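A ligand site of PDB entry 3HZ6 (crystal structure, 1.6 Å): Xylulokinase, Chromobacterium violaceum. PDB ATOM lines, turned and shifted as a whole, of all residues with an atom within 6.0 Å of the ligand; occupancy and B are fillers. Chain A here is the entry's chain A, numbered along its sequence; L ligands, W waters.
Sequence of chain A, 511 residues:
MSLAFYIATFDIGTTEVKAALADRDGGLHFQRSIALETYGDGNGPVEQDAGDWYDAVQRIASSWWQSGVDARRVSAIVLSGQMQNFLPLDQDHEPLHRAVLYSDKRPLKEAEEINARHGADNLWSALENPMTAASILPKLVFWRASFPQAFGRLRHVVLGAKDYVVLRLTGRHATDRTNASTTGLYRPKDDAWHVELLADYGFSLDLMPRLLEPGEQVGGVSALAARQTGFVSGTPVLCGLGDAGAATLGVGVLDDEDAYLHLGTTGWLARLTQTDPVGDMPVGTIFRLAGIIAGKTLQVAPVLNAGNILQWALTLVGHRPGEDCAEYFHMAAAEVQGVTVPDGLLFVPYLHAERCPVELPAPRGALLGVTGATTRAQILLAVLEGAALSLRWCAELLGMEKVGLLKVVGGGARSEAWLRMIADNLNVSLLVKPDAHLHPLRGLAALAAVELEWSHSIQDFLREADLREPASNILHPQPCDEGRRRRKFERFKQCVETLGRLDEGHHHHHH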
ATOM      1  N   HIS A 262       5.160  14.289  27.267  1.00  0.00           N
ATOM      2  CA  HIS A 262       4.109  13.675  26.451  1.00  0.00           C
ATOM      3  C   HIS A 262       4.628  13.615  25.018  1.00  0.00           C
ATOM      4  O   HIS A 262       4.840  14.659  24.435  1.00  0.00           O
ATOM      5  CB  HIS A 262       2.833  14.504  26.523  1.00  0.00           C
ATOM      6  CG  HIS A 262       1.701  13.857  25.799  1.00  0.00           C
ATOM      7  ND1 HIS A 262       0.683  13.208  26.466  1.00  0.00           N
ATOM      8  CD2 HIS A 262       1.447  13.711  24.481  1.00  0.00           C
ATOM      9  CE1 HIS A 262      -0.157  12.697  25.571  1.00  0.00           C
ATOM     10  NE2 HIS A 262       0.289  12.996  24.362  1.00  0.00           N
ATOM     11  N   LEU A 263       4.853  12.408  24.514  1.00  0.00           N
ATOM     12  CA  LEU A 263       5.352  12.179  23.157  1.00  0.00           C
ATOM     13  C   LEU A 263       4.211  11.667  22.311  1.00  0.00           C
ATOM     14  O   LEU A 263       4.127  10.467  22.043  1.00  0.00           O
ATOM     15  CB  LEU A 263       6.463  11.123  23.161  1.00  0.00           C
ATOM     16  CG  LEU A 263       7.793  11.501  23.805  1.00  0.00           C
ATOM     17  CD1 LEU A 263       8.833  10.407  23.580  1.00  0.00           C
ATOM     18  CD2 LEU A 263       8.281  12.816  23.217  1.00  0.00           C
ATOM     19  N   GLY A 264       3.302  12.526  21.913  1.00  0.00           N
ATOM     20  CA  GLY A 264       2.283  12.107  20.984  1.00  0.00           C
ATOM     21  C   GLY A 264       2.658  12.636  19.608  1.00  0.00           C
ATOM     22  O   GLY A 264       3.821  12.942  19.385  1.00  0.00           O
ATOM     23  N   THR A 265       1.680  12.765  18.719  1.00  0.00           N
ATOM     24  CA  THR A 265       1.919  13.389  17.429  1.00  0.00           C
ATOM     25  C   THR A 265       2.520  14.773  17.650  1.00  0.00           C
ATOM     26  O   THR A 265       3.511  15.144  17.025  1.00  0.00           O
ATOM     27  CB  THR A 265       0.588  13.476  16.666  1.00  0.00           C
ATOM     28  OG1 THR A 265       0.173  12.132  16.405  1.00  0.00           O
ATOM     29  CG2 THR A 265       0.764  14.210  15.366  1.00  0.00           C
ATOM     30  N   THR A 266       1.909  15.516  18.568  1.00  0.00           N
ATOM     31  CA  THR A 266       2.538  16.720  19.106  1.00  0.00           C
ATOM     32  C   THR A 266       2.773  16.360  20.568  1.00  0.00           C
ATOM     33  O   THR A 266       2.294  15.319  21.011  1.00  0.00           O
ATOM     34  CB  THR A 266       1.675  17.965  19.020  1.00  0.00           C
ATOM     35  OG1 THR A 266       0.420  17.710  19.686  1.00  0.00           O
ATOM     36  CG2 THR A 266       1.381  18.331  17.575  1.00  0.00           C
ATOM     37  N   ALA A 306       6.946  16.521  17.188  1.00  0.00           N
ATOM     38  CA  ALA A 306       7.284  15.452  18.126  1.00  0.00           C
ATOM     39  C   ALA A 306       7.084  14.124  17.406  1.00  0.00           C
ATOM     40  O   ALA A 306       7.862  13.791  16.516  1.00  0.00           O
ATOM     41  CB  ALA A 306       6.389  15.560  19.378  1.00  0.00           C
ATOM     42  N   GLY A 307       6.064  13.365  17.759  1.00  0.00           N
ATOM     43  CA  GLY A 307       5.828  12.073  17.133  1.00  0.00           C
ATOM     44  C   GLY A 307       5.601  12.198  15.648  1.00  0.00           C
ATOM     45  O   GLY A 307       5.890  11.285  14.906  1.00  0.00           O
ATOM     46  N   ASN A 308       5.061  13.331  15.228  1.00  0.00           N
ATOM     47  CA  ASN A 308       4.810  13.516  13.810  1.00  0.00           C
ATOM     48  C   ASN A 308       6.091  13.518  13.011  1.00  0.00           C
ATOM     49  O   ASN A 308       6.042  13.255  11.811  1.00  0.00           O
ATOM     50  CB  ASN A 308       3.981  14.765  13.535  1.00  0.00           C
ATOM     51  CG  ASN A 308       4.501  16.005  14.246  1.00  0.00           C
ATOM     52  OD1 ASN A 308       5.631  16.046  14.769  1.00  0.00           O
ATOM     53  ND2 ASN A 308       3.659  17.028  14.261  1.00  0.00           N
ATOM     54  N   ILE A 309       7.223  13.770  13.664  1.00  0.00           N
ATOM     55  CA  ILE A 309       8.505  13.766  12.947  1.00  0.00           C
ATOM     56  C   ILE A 309       8.877  12.305  12.597  1.00  0.00           C
ATOM     57  O   ILE A 309       9.373  12.007  11.483  1.00  0.00           O
ATOM     58  CB  ILE A 309       9.593  14.367  13.819  1.00  0.00           C
ATOM     59  CG1 ILE A 309       9.298  15.852  14.075  1.00  0.00           C
ATOM     60  CG2 ILE A 309      10.959  14.192  13.167  1.00  0.00           C
ATOM     61  CD1 ILE A 309       8.963  16.596  12.814  1.00  0.00           C
ATOM     62  N   LEU A 310       8.693  11.395  13.548  1.00  0.00           N
ATOM     63  CA  LEU A 310       8.958   9.971  13.309  1.00  0.00           C
ATOM     64  C   LEU A 310       8.006   9.419  12.271  1.00  0.00           C
ATOM     65  O   LEU A 310       8.386   8.614  11.422  1.00  0.00           O
ATOM     66  CB  LEU A 310       8.820   9.160  14.598  1.00  0.00           C
ATOM     67  CG  LEU A 310      10.019   9.219  15.510  1.00  0.00           C
ATOM     68  CD1 LEU A 310      10.331  10.613  16.080  1.00  0.00           C
ATOM     69  CD2 LEU A 310       9.787   8.223  16.652  1.00  0.00           C
ATOM     70  N   GLN A 311       6.746   9.870  12.327  1.00  0.00           N
ATOM     71  CA  GLN A 311       5.758   9.435  11.361  1.00  0.00           C
ATOM     72  C   GLN A 311       6.169   9.893   9.955  1.00  0.00           C
ATOM     73  O   GLN A 311       6.051   9.126   8.975  1.00  0.00           O
ATOM     74  CB  GLN A 311       4.418  10.032  11.746  1.00  0.00           C
ATOM     75  CG  GLN A 311       3.218   9.325  11.170  1.00  0.00           C
ATOM     76  CD  GLN A 311       2.129   9.212  12.244  1.00  0.00           C
ATOM     77  OE1 GLN A 311       1.533   8.131  12.442  1.00  0.00           O
ATOM     78  NE2 GLN A 311       1.886  10.318  12.964  1.00  0.00           N
ATOM     79  N   ALA A 326       2.415   0.315  10.696  1.00  0.00           N
ATOM     80  CA  ALA A 326       3.032  -0.615  11.640  1.00  0.00           C
ATOM     81  C   ALA A 326       4.313  -1.231  11.132  1.00  0.00           C
ATOM     82  O   ALA A 326       5.332  -1.260  11.824  1.00  0.00           O
ATOM     83  CB  ALA A 326       2.062  -1.731  12.020  1.00  0.00           C
ATOM     84  N   PHE A 329       7.173   1.318  10.907  1.00  0.00           N
ATOM     85  CA  PHE A 329       7.829   1.611  12.191  1.00  0.00           C
ATOM     86  C   PHE A 329       8.765   0.476  12.574  1.00  0.00           C
ATOM     87  O   PHE A 329       9.867   0.700  13.090  1.00  0.00           O
ATOM     88  CB  PHE A 329       6.807   1.836  13.347  1.00  0.00           C
ATOM     89  CG  PHE A 329       6.177   3.195  13.358  1.00  0.00           C
ATOM     90  CD1 PHE A 329       6.952   4.322  13.648  1.00  0.00           C
ATOM     91  CD2 PHE A 329       4.821   3.358  13.130  1.00  0.00           C
ATOM     92  CE1 PHE A 329       6.380   5.548  13.685  1.00  0.00           C
ATOM     93  CE2 PHE A 329       4.262   4.605  13.149  1.00  0.00           C
ATOM     94  CZ  PHE A 329       5.050   5.707  13.433  1.00  0.00           C
ATOM     95  N   HIS A 330       8.329  -0.747  12.333  1.00  0.00           N
ATOM     96  CA  HIS A 330       9.182  -1.886  12.610  1.00  0.00           C
ATOM     97  C   HIS A 330      10.493  -1.833  11.831  1.00  0.00           C
ATOM     98  O   HIS A 330      11.585  -2.067  12.396  1.00  0.00           O
ATOM     99  CB  HIS A 330       8.412  -3.181  12.291  1.00  0.00           C
ATOM    100  CG  HIS A 330       9.180  -4.432  12.581  1.00  0.00           C
ATOM    101  ND1 HIS A 330       9.380  -4.907  13.864  1.00  0.00           N
ATOM    102  CD2 HIS A 330       9.785  -5.310  11.756  1.00  0.00           C
ATOM    103  CE1 HIS A 330      10.090  -6.027  13.809  1.00  0.00           C
ATOM    104  NE2 HIS A 330      10.346  -6.296  12.538  1.00  0.00           N
ATOM    105  N   VAL A 409       5.050   9.604  28.487  1.00  0.00           N
ATOM    106  CA  VAL A 409       3.795   9.003  28.022  1.00  0.00           C
ATOM    107  C   VAL A 409       3.637   9.242  26.546  1.00  0.00           C
ATOM    108  O   VAL A 409       4.274  10.113  25.976  1.00  0.00           O
ATOM    109  CB  VAL A 409       2.606   9.564  28.807  1.00  0.00           C
ATOM    110  CG1 VAL A 409       2.864   9.423  30.317  1.00  0.00           C
ATOM    111  CG2 VAL A 409       2.371  10.987  28.456  1.00  0.00           C
ATOM    112  N   GLY A 410       2.810   8.438  25.912  1.00  0.00           N
ATOM    113  CA  GLY A 410       2.412   8.694  24.556  1.00  0.00           C
ATOM    114  C   GLY A 410       2.986   7.714  23.545  1.00  0.00           C
ATOM    115  O   GLY A 410       3.905   6.966  23.854  1.00  0.00           O
ATOM    116  N   GLY A 411       2.429   7.725  22.342  1.00  0.00           N
ATOM    117  CA  GLY A 411       2.799   6.725  21.356  1.00  0.00           C
ATOM    118  C   GLY A 411       4.220   6.844  20.860  1.00  0.00           C
ATOM    119  O   GLY A 411       4.808   5.841  20.431  1.00  0.00           O
ATOM    120  N   GLY A 412       4.798   8.026  20.945  1.00  0.00           N
ATOM    121  CA  GLY A 412       6.197   8.169  20.590  1.00  0.00           C
ATOM    122  C   GLY A 412       7.109   7.301  21.408  1.00  0.00           C
ATOM    123  O   GLY A 412       8.184   6.925  20.923  1.00  0.00           O
ATOM    124  N   ALA A 413       6.715   6.976  22.658  1.00  0.00           N
ATOM    125  CA  ALA A 413       7.533   6.153  23.526  1.00  0.00           C
ATOM    126  C   ALA A 413       7.660   4.712  23.069  1.00  0.00           C
ATOM    127  O   ALA A 413       8.448   3.963  23.617  1.00  0.00           O
ATOM    128  CB  ALA A 413       7.026   6.203  24.985  1.00  0.00           C
ATOM    129  N   ARG A 414       6.925   4.346  22.023  1.00  0.00           N
ATOM    130  CA  ARG A 414       7.087   3.032  21.406  1.00  0.00           C
ATOM    131  C   ARG A 414       8.437   2.939  20.693  1.00  0.00           C
ATOM    132  O   ARG A 414       8.911   1.841  20.396  1.00  0.00           O
ATOM    133  CB  ARG A 414       5.937   2.686  20.445  1.00  0.00           C
ATOM    134  CG  ARG A 414       4.573   2.523  21.111  1.00  0.00           C
ATOM    135  CD  ARG A 414       3.547   2.156  20.040  1.00  0.00           C
ATOM    136  NE  ARG A 414       2.184   2.414  20.484  1.00  0.00           N
ATOM    137  CZ  ARG A 414       1.122   2.361  19.684  1.00  0.00           C
ATOM    138  NH1 ARG A 414       1.276   2.044  18.401  1.00  0.00           N
ATOM    139  NH2 ARG A 414      -0.089   2.613  20.164  1.00  0.00           N
ATOM    140  N   SER A 415       9.047   4.091  20.386  1.00  0.00           N
ATOM    141  CA  SER A 415      10.369   4.034  19.756  1.00  0.00           C
ATOM    142  C   SER A 415      11.479   3.919  20.780  1.00  0.00           C
ATOM    143  O   SER A 415      11.833   4.892  21.445  1.00  0.00           O
ATOM    144  CB  SER A 415      10.587   5.239  18.838  1.00  0.00           C
ATOM    145  OG  SER A 415      11.951   5.296  18.374  1.00  0.00           O
HETATM  146  P1  LIG L   1      -1.775  11.492  19.262  1.00  0.00           P
HETATM  147  O1  LIG L   1      -3.004  11.131  20.097  1.00  0.00           O
HETATM  148  O2  LIG L   1      -1.859  11.042  17.817  1.00  0.00           O
HETATM  149  O3  LIG L   1      -1.342  12.949  19.413  1.00  0.00           O
HETATM  150  P2  LIG L   1      -0.268   9.246  20.336  1.00  0.00           P
HETATM  151  O4  LIG L   1      -0.003   9.173  21.820  1.00  0.00           O
HETATM  152  O5  LIG L   1      -1.365   8.498  19.627  1.00  0.00           O
HETATM  153  O6  LIG L   1      -0.492  10.805  19.984  1.00  0.00           O
HETATM  154  O7  LIG L   1       1.108   9.024  19.519  1.00  0.00           O
HETATM  155  C1  LIG L   1       1.151   9.096  18.099  1.00  0.00           C
HETATM  156  C2  LIG L   1       2.606   8.934  17.772  1.00  0.00           C
HETATM  157  O8  LIG L   1       3.028   7.612  18.098  1.00  0.00           O
HETATM  158  C3  LIG L   1       2.766   9.042  16.288  1.00  0.00           C
HETATM  159  O9  LIG L   1       3.267  10.318  15.979  1.00  0.00           O
HETATM  160  C4  LIG L   1       3.748   7.975  15.920  1.00  0.00           C
HETATM  161  O10 LIG L   1       4.931   8.603  15.450  1.00  0.00           O
HETATM  162  C5  LIG L   1       4.091   7.246  17.204  1.00  0.00           C
HETATM  163  N1  LIG L   1       4.019   5.800  16.961  1.00  0.00           N
HETATM  164  C6  LIG L   1       2.914   5.082  16.599  1.00  0.00           C
HETATM  165  N2  LIG L   1       3.218   3.766  16.454  1.00  0.00           N
HETATM  166  C7  LIG L   1       4.553   3.660  16.707  1.00  0.00           C
HETATM  167  C8  LIG L   1       5.558   2.576  16.766  1.00  0.00           C
HETATM  168  N3  LIG L   1       5.207   1.310  16.486  1.00  0.00           N
HETATM  169  N4  LIG L   1       6.830   2.911  17.075  1.00  0.00           N
HETATM  170  C9  LIG L   1       7.195   4.181  17.364  1.00  0.00           C
HETATM  171  N5  LIG L   1       6.330   5.220  17.344  1.00  0.00           N
HETATM  172  C10 LIG L   1       5.051   4.993  17.040  1.00  0.00           C
HETATM  173  O   HOH W   1      -3.469  13.016  16.123  1.00  0.00           O
HETATM  174  O   HOH W   2       9.255   1.756  17.058  1.00  0.00           O
HETATM  175  O   HOH W   3      -1.137  12.478  21.872  1.00  0.00           O
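Water W3 bridges an oxygen (O3) of the ligand (2.5 Å) and a ring nitrogen (NE2) of His 262 (2.9 Å). Water W2 lies within hydrogen-bond range of a nitrogen (N4) of the ligand (2.7 Å) and the backbone carbonyl oxygen of Arg 414 (3.4 Å).
N of Gly 307 lies within hydrogen-bond range of O of Thr 265, 3.2 Å away. The backbone carbonyl oxygen of Thr 265 lies within hydrogen-bond range of the backbone NH of Asn 308. The backbone carbonyl oxygen of Leu 263 lies within hydrogen-bond range of the backbone NH of Gly 411, at 3.2 Å. The backbone carbonyl oxygen (O) of Gly 264 lies within hydrogen-bond range of the backbone NH (N) of Gly 307 (2.8 Å). The backbone carbonyl oxygen (O) of Leu 263 lies within hydrogen-bond range of the backbone NH (N) of Gly 412 (2.8 Å). The side-chain amide oxygen (OD1) of Asn 308 lies within hydrogen-bond range of the backbone NH (N) of Ala 306 (2.8 Å).
Residues that only touch the ligand: Gly 264 (3.2 Å), Asn 308 (3.6 Å), Phe 329 (3.5 Å), Gly 410 (3.7 Å) and Ser 415 (3.5 Å). Within 4 Å of the ligand: Gly 264, Thr 265, Gly 307, Asn 308, Gln 311, Phe 329, Gly 410, Gly 411, Gly 412, Arg 414 and Ser 415.
O3 of the ligand lies within hydrogen-bond range of N of Thr 265 (3.1 Å). The side-chain hydroxyl (OG1) of Thr 265 sits at hydrogen-bond distance from an oxygen (O2) of the ligand, 2.7 Å away. N of Gly 411 lies within hydrogen-bond range of O4 of the ligand, 2.9 Å away. O10 of the ligand is in hydrogen-bond range of O of Gly 307 (2.9 Å). N2 of the ligand lies within hydrogen-bond range of NH1 of Arg 414 (3.2 Å). O9 of the ligand sits at hydrogen-bond distance from NE2 of Gln 311 (3.3 Å). An oxygen (O8) of the ligand is in hydrogen-bond range of the backbone NH (N) of Gly 412, at 3.4 Å.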
